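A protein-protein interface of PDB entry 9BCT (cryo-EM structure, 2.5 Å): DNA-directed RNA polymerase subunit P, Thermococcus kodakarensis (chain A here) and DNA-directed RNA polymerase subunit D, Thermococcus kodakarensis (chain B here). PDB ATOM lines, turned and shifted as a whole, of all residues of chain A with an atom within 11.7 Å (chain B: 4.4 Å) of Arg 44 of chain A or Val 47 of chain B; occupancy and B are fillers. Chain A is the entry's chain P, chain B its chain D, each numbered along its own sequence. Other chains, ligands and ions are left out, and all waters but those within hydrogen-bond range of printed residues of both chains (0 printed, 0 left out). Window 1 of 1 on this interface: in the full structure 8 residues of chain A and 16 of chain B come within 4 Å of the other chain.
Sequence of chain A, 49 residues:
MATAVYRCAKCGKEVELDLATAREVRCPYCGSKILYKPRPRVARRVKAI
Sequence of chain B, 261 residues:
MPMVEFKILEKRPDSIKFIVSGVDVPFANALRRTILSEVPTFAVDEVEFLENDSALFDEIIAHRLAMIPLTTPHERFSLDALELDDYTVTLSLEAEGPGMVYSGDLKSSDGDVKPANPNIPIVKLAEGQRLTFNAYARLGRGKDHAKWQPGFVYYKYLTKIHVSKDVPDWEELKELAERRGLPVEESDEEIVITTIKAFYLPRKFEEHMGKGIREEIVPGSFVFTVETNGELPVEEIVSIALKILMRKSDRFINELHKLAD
Hydrophobic or aromatic side chains of chain A that line the printed part of chain B: Ala 43, Val 46 and Ala 48. Of the 13 printed residues of chain B, 9 touch a printed residue of chain A. Printed residues of chain B that touch a printed residue of chain A: Val 44, Glu 46, Val 47, Glu 48, Phe 49, Leu 50, Asn 52, Asp 58 and Ala 62. Among the printed residues, Asp or Glu carboxylates within 4 Å of a Lys or Arg side-chain nitrogen of the other chain: Arg 44 of chain A with Asp 58 of chain B (3.1 Å) and Arg 45 of chain A with Glu 46 of chain B (3.2 Å).
The backbone NH of Glu 48 of chain B lies within hydrogen-bond range of the backbone carbonyl oxygen of Asn 134 of chain B (2.9 Å).
Among the printed residues, merely in contact across the chains: Arg 39 of chain A with Asn 52 of chain B (3.8 Å), Arg 41 of chain A with Leu 50 of chain B (3.5 Å), Ala 43 of chain A with Glu 48 of chain B (3.8 Å), Ala 43 of chain A with Phe 49 of chain B (3.5 Å), Ala 43 of chain A with Leu 50 of chain B (3.7 Å), Arg 44 of chain A with Val 47 of chain B (3.96 Å), Arg 44 of chain A with Glu 48 of chain B (3.3 Å), Arg 44 of chain A with Leu 50 of chain B (3.6 Å), Arg 44 of chain A with Asn 52 of chain B (3.5 Å), Arg 45 of chain A with Val 47 of chain B (3.3 Å), Arg 45 of chain A with Glu 48 of chain B (3.9 Å), Val 46 of chain A with Glu 46 of chain B (3.97 Å), Val 46 of chain A with Phe 49 of chain B (3.9 Å), Val 46 of chain A with Asp 58 of chain B (3.7 Å), Ala 48 of chain A with Val 44 of chain B (3.4 Å) and Ala 48 of chain A with Ala 62 of chain B (3.5 Å).
NH1 of Arg 45 of chain A lies within salt-bridge range of OE2 of Glu 46 of chain B, at 3.2 Å. The guanidinium group (NE) of Arg 44 of chain A lies within salt-bridge range of the side-chain carboxylate (OD2) of Asp 58 of chain B (3.1 Å). O of Val 47 of chain B lies within hydrogen-bond range of N of Val 46 of chain A (2.6 Å). O of Arg 44 of chain A lies within hydrogen-bond range of N of Phe 49 of chain B.
Of the printed residues of chain B, Arg 44 of chain A touches Val 47, Glu 48, Phe 49, Leu 50, Asn 52 and Asp 58. Of chain A, only Ala 48 comes within 4 Å of Val 44 of chain B. Of chain A, only Arg 41, Ala 43 and Arg 44 come within 4 Å of Leu 50 of chain B. Asn 52 of chain B touches just these residues of chain A: Arg 39 and Arg 44. Ala 62 of chain B touches just one residue of chain A: Ala 48 (3.5 Å). No residue of chain A comes within 4 Å of Leu 65 of chain B. Of the printed residues of chain B, Ala 48 of chain A touches Val 44 and Ala 62. Of the printed residues of chain B, Ala 43 of chain A touches Glu 48 (3.8 Å), Phe 49 (3.5 Å) and Leu 50 (3.7 Å). Lys 37 of chain A touches none of the printed residues of chain B. Lys 47 of chain A touches none of the printed residues of chain B.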
ATOM      1  N   LYS A  37      -1.190  12.099  21.080  1.00  0.00           N
ATOM      2  CA  LYS A  37      -0.533  10.804  20.980  1.00  0.00           C
ATOM      3  C   LYS A  37       0.560  10.873  19.921  1.00  0.00           C
ATOM      4  O   LYS A  37       0.265  11.186  18.761  1.00  0.00           O
ATOM      5  CB  LYS A  37      -1.538   9.716  20.630  1.00  0.00           C
ATOM      6  CG  LYS A  37      -0.998   8.304  20.782  1.00  0.00           C
ATOM      7  CD  LYS A  37      -2.124   7.299  20.960  1.00  0.00           C
ATOM      8  CE  LYS A  37      -1.585   5.883  21.090  1.00  0.00           C
ATOM      9  NZ  LYS A  37      -0.388   5.822  21.973  1.00  0.00           N
ATOM     10  N   PRO A  38       1.818  10.607  20.267  1.00  0.00           N
ATOM     11  CA  PRO A  38       2.894  10.709  19.277  1.00  0.00           C
ATOM     12  C   PRO A  38       2.777   9.646  18.196  1.00  0.00           C
ATOM     13  O   PRO A  38       2.251   8.552  18.417  1.00  0.00           O
ATOM     14  CB  PRO A  38       4.165  10.515  20.112  1.00  0.00           C
ATOM     15  CG  PRO A  38       3.715   9.737  21.300  1.00  0.00           C
ATOM     16  CD  PRO A  38       2.316  10.194  21.590  1.00  0.00           C
ATOM     17  N   ARG A  39       3.273   9.989  17.013  1.00  0.00           N
ATOM     18  CA  ARG A  39       3.241   9.058  15.897  1.00  0.00           C
ATOM     19  C   ARG A  39       4.230   7.917  16.135  1.00  0.00           C
ATOM     20  O   ARG A  39       5.359   8.154  16.576  1.00  0.00           O
ATOM     21  CB  ARG A  39       3.574   9.775  14.590  1.00  0.00           C
ATOM     22  CG  ARG A  39       2.396  10.507  13.981  1.00  0.00           C
ATOM     23  CD  ARG A  39       2.808  11.852  13.406  1.00  0.00           C
ATOM     24  NE  ARG A  39       1.862  12.324  12.403  1.00  0.00           N
ATOM     25  CZ  ARG A  39       0.700  12.901  12.679  1.00  0.00           C
ATOM     26  NH1 ARG A  39       0.308  13.105  13.925  1.00  0.00           N
ATOM     27  NH2 ARG A  39      -0.088  13.283  11.678  1.00  0.00           N
ATOM     28  N   PRO A  40       3.836   6.676  15.861  1.00  0.00           N
ATOM     29  CA  PRO A  40       4.762   5.555  16.039  1.00  0.00           C
ATOM     30  C   PRO A  40       5.889   5.600  15.020  1.00  0.00           C
ATOM     31  O   PRO A  40       5.747   6.139  13.920  1.00  0.00           O
ATOM     32  CB  PRO A  40       3.874   4.324  15.832  1.00  0.00           C
ATOM     33  CG  PRO A  40       2.764   4.809  14.967  1.00  0.00           C
ATOM     34  CD  PRO A  40       2.521   6.238  15.362  1.00  0.00           C
ATOM     35  N   ARG A  41       7.022   5.019  15.403  1.00  0.00           N
ATOM     36  CA  ARG A  41       8.207   5.003  14.558  1.00  0.00           C
ATOM     37  C   ARG A  41       8.246   3.797  13.625  1.00  0.00           C
ATOM     38  O   ARG A  41       9.205   3.646  12.863  1.00  0.00           O
ATOM     39  CB  ARG A  41       9.464   5.054  15.437  1.00  0.00           C
ATOM     40  CG  ARG A  41      10.747   5.520  14.745  1.00  0.00           C
ATOM     41  CD  ARG A  41      10.731   6.914  14.072  1.00  0.00           C
ATOM     42  NE  ARG A  41      10.363   8.029  14.945  1.00  0.00           N
ATOM     43  CZ  ARG A  41       9.137   8.497  15.149  1.00  0.00           C
ATOM     44  NH1 ARG A  41       8.113   8.114  14.405  1.00  0.00           N
ATOM     45  NH2 ARG A  41       8.946   9.424  16.083  1.00  0.00           N
ATOM     46  N   VAL A  42       7.220   2.945  13.656  1.00  0.00           N
ATOM     47  CA  VAL A  42       7.128   1.854  12.693  1.00  0.00           C
ATOM     48  C   VAL A  42       6.913   2.439  11.303  1.00  0.00           C
ATOM     49  O   VAL A  42       6.071   3.325  11.108  1.00  0.00           O
ATOM     50  CB  VAL A  42       6.006   0.880  13.088  1.00  0.00           C
ATOM     51  CG1 VAL A  42       4.732   1.634  13.448  1.00  0.00           C
ATOM     52  CG2 VAL A  42       5.744  -0.126  11.975  1.00  0.00           C
ATOM     53  N   ALA A  43       7.696   1.966  10.337  1.00  0.00           N
ATOM     54  CA  ALA A  43       7.655   2.528   8.994  1.00  0.00           C
ATOM     55  C   ALA A  43       6.317   2.236   8.327  1.00  0.00           C
ATOM     56  O   ALA A  43       5.848   1.094   8.321  1.00  0.00           O
ATOM     57  CB  ALA A  43       8.798   1.968   8.150  1.00  0.00           C
ATOM     58  N   ARG A  44       5.706   3.273   7.765  1.00  0.00           N
ATOM     59  CA  ARG A  44       4.459   3.154   7.027  1.00  0.00           C
ATOM     60  C   ARG A  44       4.719   3.454   5.558  1.00  0.00           C
ATOM     61  O   ARG A  44       5.568   4.287   5.225  1.00  0.00           O
ATOM     62  CB  ARG A  44       3.388   4.100   7.584  1.00  0.00           C
ATOM     63  CG  ARG A  44       3.728   5.578   7.473  1.00  0.00           C
ATOM     64  CD  ARG A  44       3.859   6.223   8.842  1.00  0.00           C
ATOM     65  NE  ARG A  44       3.770   7.676   8.767  1.00  0.00           N
ATOM     66  CZ  ARG A  44       4.452   8.509   9.542  1.00  0.00           C
ATOM     67  NH1 ARG A  44       5.285   8.064  10.468  1.00  0.00           N
ATOM     68  NH2 ARG A  44       4.293   9.819   9.385  1.00  0.00           N
ATOM     69  N   ARG A  45       4.000   2.762   4.682  1.00  0.00           N
ATOM     70  CA  ARG A  45       4.189   2.886   3.243  1.00  0.00           C
ATOM     71  C   ARG A  45       2.972   3.575   2.642  1.00  0.00           C
ATOM     72  O   ARG A  45       1.839   3.122   2.835  1.00  0.00           O
ATOM     73  CB  ARG A  45       4.410   1.519   2.601  1.00  0.00           C
ATOM     74  CG  ARG A  45       4.605   1.576   1.101  1.00  0.00           C
ATOM     75  CD  ARG A  45       6.082   1.566   0.748  1.00  0.00           C
ATOM     76  NE  ARG A  45       6.811   0.539   1.482  1.00  0.00           N
ATOM     77  CZ  ARG A  45       7.486  -0.451   0.914  1.00  0.00           C
ATOM     78  NH1 ARG A  45       7.546  -0.580  -0.401  1.00  0.00           N
ATOM     79  NH2 ARG A  45       8.115  -1.333   1.684  1.00  0.00           N
ATOM     80  N   VAL A  46       3.210   4.664   1.915  1.00  0.00           N
ATOM     81  CA  VAL A  46       2.155   5.458   1.299  1.00  0.00           C
ATOM     82  C   VAL A  46       2.370   5.453  -0.207  1.00  0.00           C
ATOM     83  O   VAL A  46       3.465   5.772  -0.684  1.00  0.00           O
ATOM     84  CB  VAL A  46       2.136   6.898   1.842  1.00  0.00           C
ATOM     85  CG1 VAL A  46       1.059   7.717   1.149  1.00  0.00           C
ATOM     86  CG2 VAL A  46       1.923   6.893   3.348  1.00  0.00           C
ATOM     87  N   LYS A  47       1.328   5.087  -0.951  1.00  0.00           N
ATOM     88  CA  LYS A  47       1.407   5.086  -2.404  1.00  0.00           C
ATOM     89  C   LYS A  47       1.451   6.516  -2.928  1.00  0.00           C
ATOM     90  O   LYS A  47       0.668   7.370  -2.501  1.00  0.00           O
ATOM     91  CB  LYS A  47       0.215   4.340  -3.000  1.00  0.00           C
ATOM     92  CG  LYS A  47       0.534   3.575  -4.276  1.00  0.00           C
ATOM     93  CD  LYS A  47      -0.520   2.516  -4.580  1.00  0.00           C
ATOM     94  CE  LYS A  47      -0.978   1.792  -3.322  1.00  0.00           C
ATOM     95  NZ  LYS A  47       0.062   0.859  -2.809  1.00  0.00           N
ATOM     96  N   ALA A  48       2.369   6.777  -3.855  1.00  0.00           N
ATOM     97  CA  ALA A  48       2.528   8.108  -4.435  1.00  0.00           C
ATOM     98  C   ALA A  48       1.403   8.334  -5.437  1.00  0.00           C
ATOM     99  O   ALA A  48       1.463   7.856  -6.572  1.00  0.00           O
ATOM    100  CB  ALA A  48       3.896   8.250  -5.091  1.00  0.00           C
ATOM    101  N   ILE A  49       0.378   9.070  -5.006  1.00  0.00           N
ATOM    102  CA  ILE A  49      -0.805   9.375  -5.813  1.00  0.00           C
ATOM    103  C   ILE A  49      -1.474   8.102  -6.325  1.00  0.00           C
ATOM    104  O   ILE A  49      -1.302   7.721  -7.482  1.00  0.00           O
ATOM    105  CB  ILE A  49      -0.458  10.318  -6.984  1.00  0.00           C
ATOM    106  N   VAL B  44       8.721   8.637  -8.862  1.00  0.00           N
ATOM    107  CA  VAL B  44       8.537   8.025  -7.551  1.00  0.00           C
ATOM    108  C   VAL B  44       7.188   7.321  -7.520  1.00  0.00           C
ATOM    109  O   VAL B  44       6.138   7.949  -7.693  1.00  0.00           O
ATOM    110  CB  VAL B  44       8.646   9.072  -6.435  1.00  0.00           C
ATOM    111  CG1 VAL B  44       8.129   8.506  -5.123  1.00  0.00           C
ATOM    112  CG2 VAL B  44      10.085   9.541  -6.290  1.00  0.00           C
ATOM    113  N   GLU B  46       6.420   4.658  -4.945  1.00  0.00           N
ATOM    114  CA  GLU B  46       6.042   4.289  -3.589  1.00  0.00           C
ATOM    115  C   GLU B  46       6.876   5.099  -2.609  1.00  0.00           C
ATOM    116  O   GLU B  46       7.990   5.516  -2.926  1.00  0.00           O
ATOM    117  CB  GLU B  46       6.242   2.783  -3.363  1.00  0.00           C
ATOM    118  CG  GLU B  46       5.044   2.069  -2.762  1.00  0.00           C
ATOM    119  CD  GLU B  46       5.300   0.586  -2.560  1.00  0.00           C
ATOM    120  OE1 GLU B  46       6.150   0.028  -3.285  1.00  0.00           O
ATOM    121  OE2 GLU B  46       4.641  -0.025  -1.694  1.00  0.00           O
ATOM    122  N   VAL B  47       6.324   5.353  -1.426  1.00  0.00           N
ATOM    123  CA  VAL B  47       7.024   6.108  -0.391  1.00  0.00           C
ATOM    124  C   VAL B  47       6.855   5.386   0.938  1.00  0.00           C
ATOM    125  O   VAL B  47       5.728   5.090   1.347  1.00  0.00           O
ATOM    126  CB  VAL B  47       6.513   7.558  -0.281  1.00  0.00           C
ATOM    127  CG1 VAL B  47       7.194   8.268   0.875  1.00  0.00           C
ATOM    128  CG2 VAL B  47       6.751   8.320  -1.577  1.00  0.00           C
ATOM    129  N   GLU B  48       7.971   5.110   1.610  1.00  0.00           N
ATOM    130  CA  GLU B  48       7.971   4.566   2.961  1.00  0.00           C
ATOM    131  C   GLU B  48       8.373   5.682   3.916  1.00  0.00           C
ATOM    132  O   GLU B  48       9.469   6.239   3.797  1.00  0.00           O
ATOM    133  CB  GLU B  48       8.926   3.378   3.076  1.00  0.00           C
ATOM    134  CG  GLU B  48       9.304   3.018   4.502  1.00  0.00           C
ATOM    135  CD  GLU B  48      10.518   2.112   4.569  1.00  0.00           C
ATOM    136  OE1 GLU B  48      10.413   0.941   4.150  1.00  0.00           O
ATOM    137  OE2 GLU B  48      11.579   2.572   5.041  1.00  0.00           O
ATOM    138  N   PHE B  49       7.492   6.000   4.860  1.00  0.00           N
ATOM    139  CA  PHE B  49       7.665   7.143   5.744  1.00  0.00           C
ATOM    140  C   PHE B  49       8.164   6.684   7.108  1.00  0.00           C
ATOM    141  O   PHE B  49       7.569   5.797   7.727  1.00  0.00           O
ATOM    142  CB  PHE B  49       6.353   7.913   5.900  1.00  0.00           C
ATOM    143  CG  PHE B  49       6.185   9.030   4.913  1.00  0.00           C
ATOM    144  CD1 PHE B  49       7.031  10.124   4.935  1.00  0.00           C
ATOM    145  CD2 PHE B  49       5.177   8.989   3.964  1.00  0.00           C
ATOM    146  CE1 PHE B  49       6.878  11.155   4.029  1.00  0.00           C
ATOM    147  CE2 PHE B  49       5.017  10.016   3.057  1.00  0.00           C
ATOM    148  CZ  PHE B  49       5.870  11.100   3.088  1.00  0.00           C
ATOM    149  N   LEU B  50       9.255   7.295   7.568  1.00  0.00           N
ATOM    150  CA  LEU B  50       9.783   7.067   8.907  1.00  0.00           C
ATOM    151  C   LEU B  50       9.328   8.138   9.892  1.00  0.00           C
ATOM    152  O   LEU B  50       8.847   7.817  10.982  1.00  0.00           O
ATOM    153  CB  LEU B  50      11.315   7.008   8.870  1.00  0.00           C
ATOM    154  CG  LEU B  50      11.960   5.648   8.586  1.00  0.00           C
ATOM    155  CD1 LEU B  50      11.248   4.540   9.349  1.00  0.00           C
ATOM    156  CD2 LEU B  50      11.977   5.354   7.093  1.00  0.00           C
ATOM    157  N   ASN B  52       7.313  12.169   9.906  1.00  0.00           N
ATOM    158  CA  ASN B  52       6.661  13.248   9.164  1.00  0.00           C
ATOM    159  C   ASN B  52       5.931  14.129  10.174  1.00  0.00           C
ATOM    160  O   ASN B  52       4.822  13.797  10.604  1.00  0.00           O
ATOM    161  CB  ASN B  52       5.708  12.699   8.111  1.00  0.00           C
ATOM    162  CG  ASN B  52       5.124  13.789   7.233  1.00  0.00           C
ATOM    163  OD1 ASN B  52       5.683  14.878   7.120  1.00  0.00           O
ATOM    164  ND2 ASN B  52       3.989  13.499   6.607  1.00  0.00           N
ATOM    165  N   ASP B  58       1.068  12.784   4.513  1.00  0.00           N
ATOM    166  CA  ASP B  58       1.889  11.778   3.846  1.00  0.00           C
ATOM    167  C   ASP B  58       1.530  11.660   2.370  1.00  0.00           C
ATOM    168  O   ASP B  58       2.417  11.558   1.514  1.00  0.00           O
ATOM    169  CB  ASP B  58       1.732  10.427   4.544  1.00  0.00           C
ATOM    170  CG  ASP B  58       2.570  10.319   5.801  1.00  0.00           C
ATOM    171  OD1 ASP B  58       3.261  11.301   6.142  1.00  0.00           O
ATOM    172  OD2 ASP B  58       2.539   9.251   6.446  1.00  0.00           O
ATOM    173  N   ALA B  62       3.996  12.474  -0.751  1.00  0.00           N
ATOM    174  CA  ALA B  62       4.248  11.413  -1.721  1.00  0.00           C
ATOM    175  C   ALA B  62       3.892  11.854  -3.135  1.00  0.00           C
ATOM    176  O   ALA B  62       4.630  11.570  -4.087  1.00  0.00           O
ATOM    177  CB  ALA B  62       3.466  10.156  -1.338  1.00  0.00           C
ATOM    178  N   LEU B  65       6.522  14.240  -4.359  1.00  0.00           N
ATOM    179  CA  LEU B  65       7.702  13.482  -4.762  1.00  0.00           C
ATOM    180  C   LEU B  65       7.491  12.809  -6.112  1.00  0.00           C
ATOM    181  O   LEU B  65       8.423  12.725  -6.921  1.00  0.00           O
ATOM    182  CB  LEU B  65       8.047  12.442  -3.697  1.00  0.00           C
ATOM    183  CG  LEU B  65       8.641  12.968  -2.392  1.00  0.00           C
ATOM    184  CD1 LEU B  65       8.298  12.030  -1.248  1.00  0.00           C
ATOM    185  CD2 LEU B  65      10.144  13.143  -2.519  1.00  0.00           C
ATOM    186  N   PHE B 133      12.149   9.805   4.963  1.00  0.00           N
ATOM    187  CA  PHE B 133      11.450   8.816   4.153  1.00  0.00           C
ATOM    188  C   PHE B 133      12.403   8.203   3.136  1.00  0.00           C
ATOM    189  O   PHE B 133      13.516   8.690   2.912  1.00  0.00           O
ATOM    190  CB  PHE B 133      10.223   9.417   3.450  1.00  0.00           C
ATOM    191  CG  PHE B 133      10.524  10.622   2.597  1.00  0.00           C
ATOM    192  CD1 PHE B 133      11.059  10.482   1.326  1.00  0.00           C
ATOM    193  CD2 PHE B 133      10.238  11.894   3.057  1.00  0.00           C
ATOM    194  CE1 PHE B 133      11.330  11.586   0.545  1.00  0.00           C
ATOM    195  CE2 PHE B 133      10.498  13.001   2.278  1.00  0.00           C
ATOM    196  CZ  PHE B 133      11.046  12.847   1.021  1.00  0.00           C
ATOM    197  N   ASN B 134      11.938   7.112   2.529  1.00  0.00           N
ATOM    198  CA  ASN B 134      12.598   6.475   1.397  1.00  0.00           C
ATOM    199  C   ASN B 134      11.592   6.371   0.261  1.00  0.00           C
ATOM    200  O   ASN B 134      10.532   5.758   0.423  1.00  0.00           O
ATOM    201  CB  ASN B 134      13.129   5.087   1.770  1.00  0.00           C
ATOM    202  CG  ASN B 134      14.084   5.122   2.945  1.00  0.00           C
ATOM    203  OD1 ASN B 134      15.008   5.933   2.985  1.00  0.00           O
ATOM    204  ND2 ASN B 134      13.865   4.238   3.911  1.00  0.00           N
ATOM    205  N   ALA B 135      11.919   6.963  -0.883  1.00  0.00           N
ATOM    206  CA  ALA B 135      11.049   6.952  -2.049  1.00  0.00           C
ATOM    207  C   ALA B 135      11.573   5.932  -3.052  1.00  0.00           C
ATOM    208  O   ALA B 135      12.720   6.028  -3.499  1.00  0.00           O
ATOM    209  CB  ALA B 135      10.968   8.341  -2.683  1.00  0.00           C
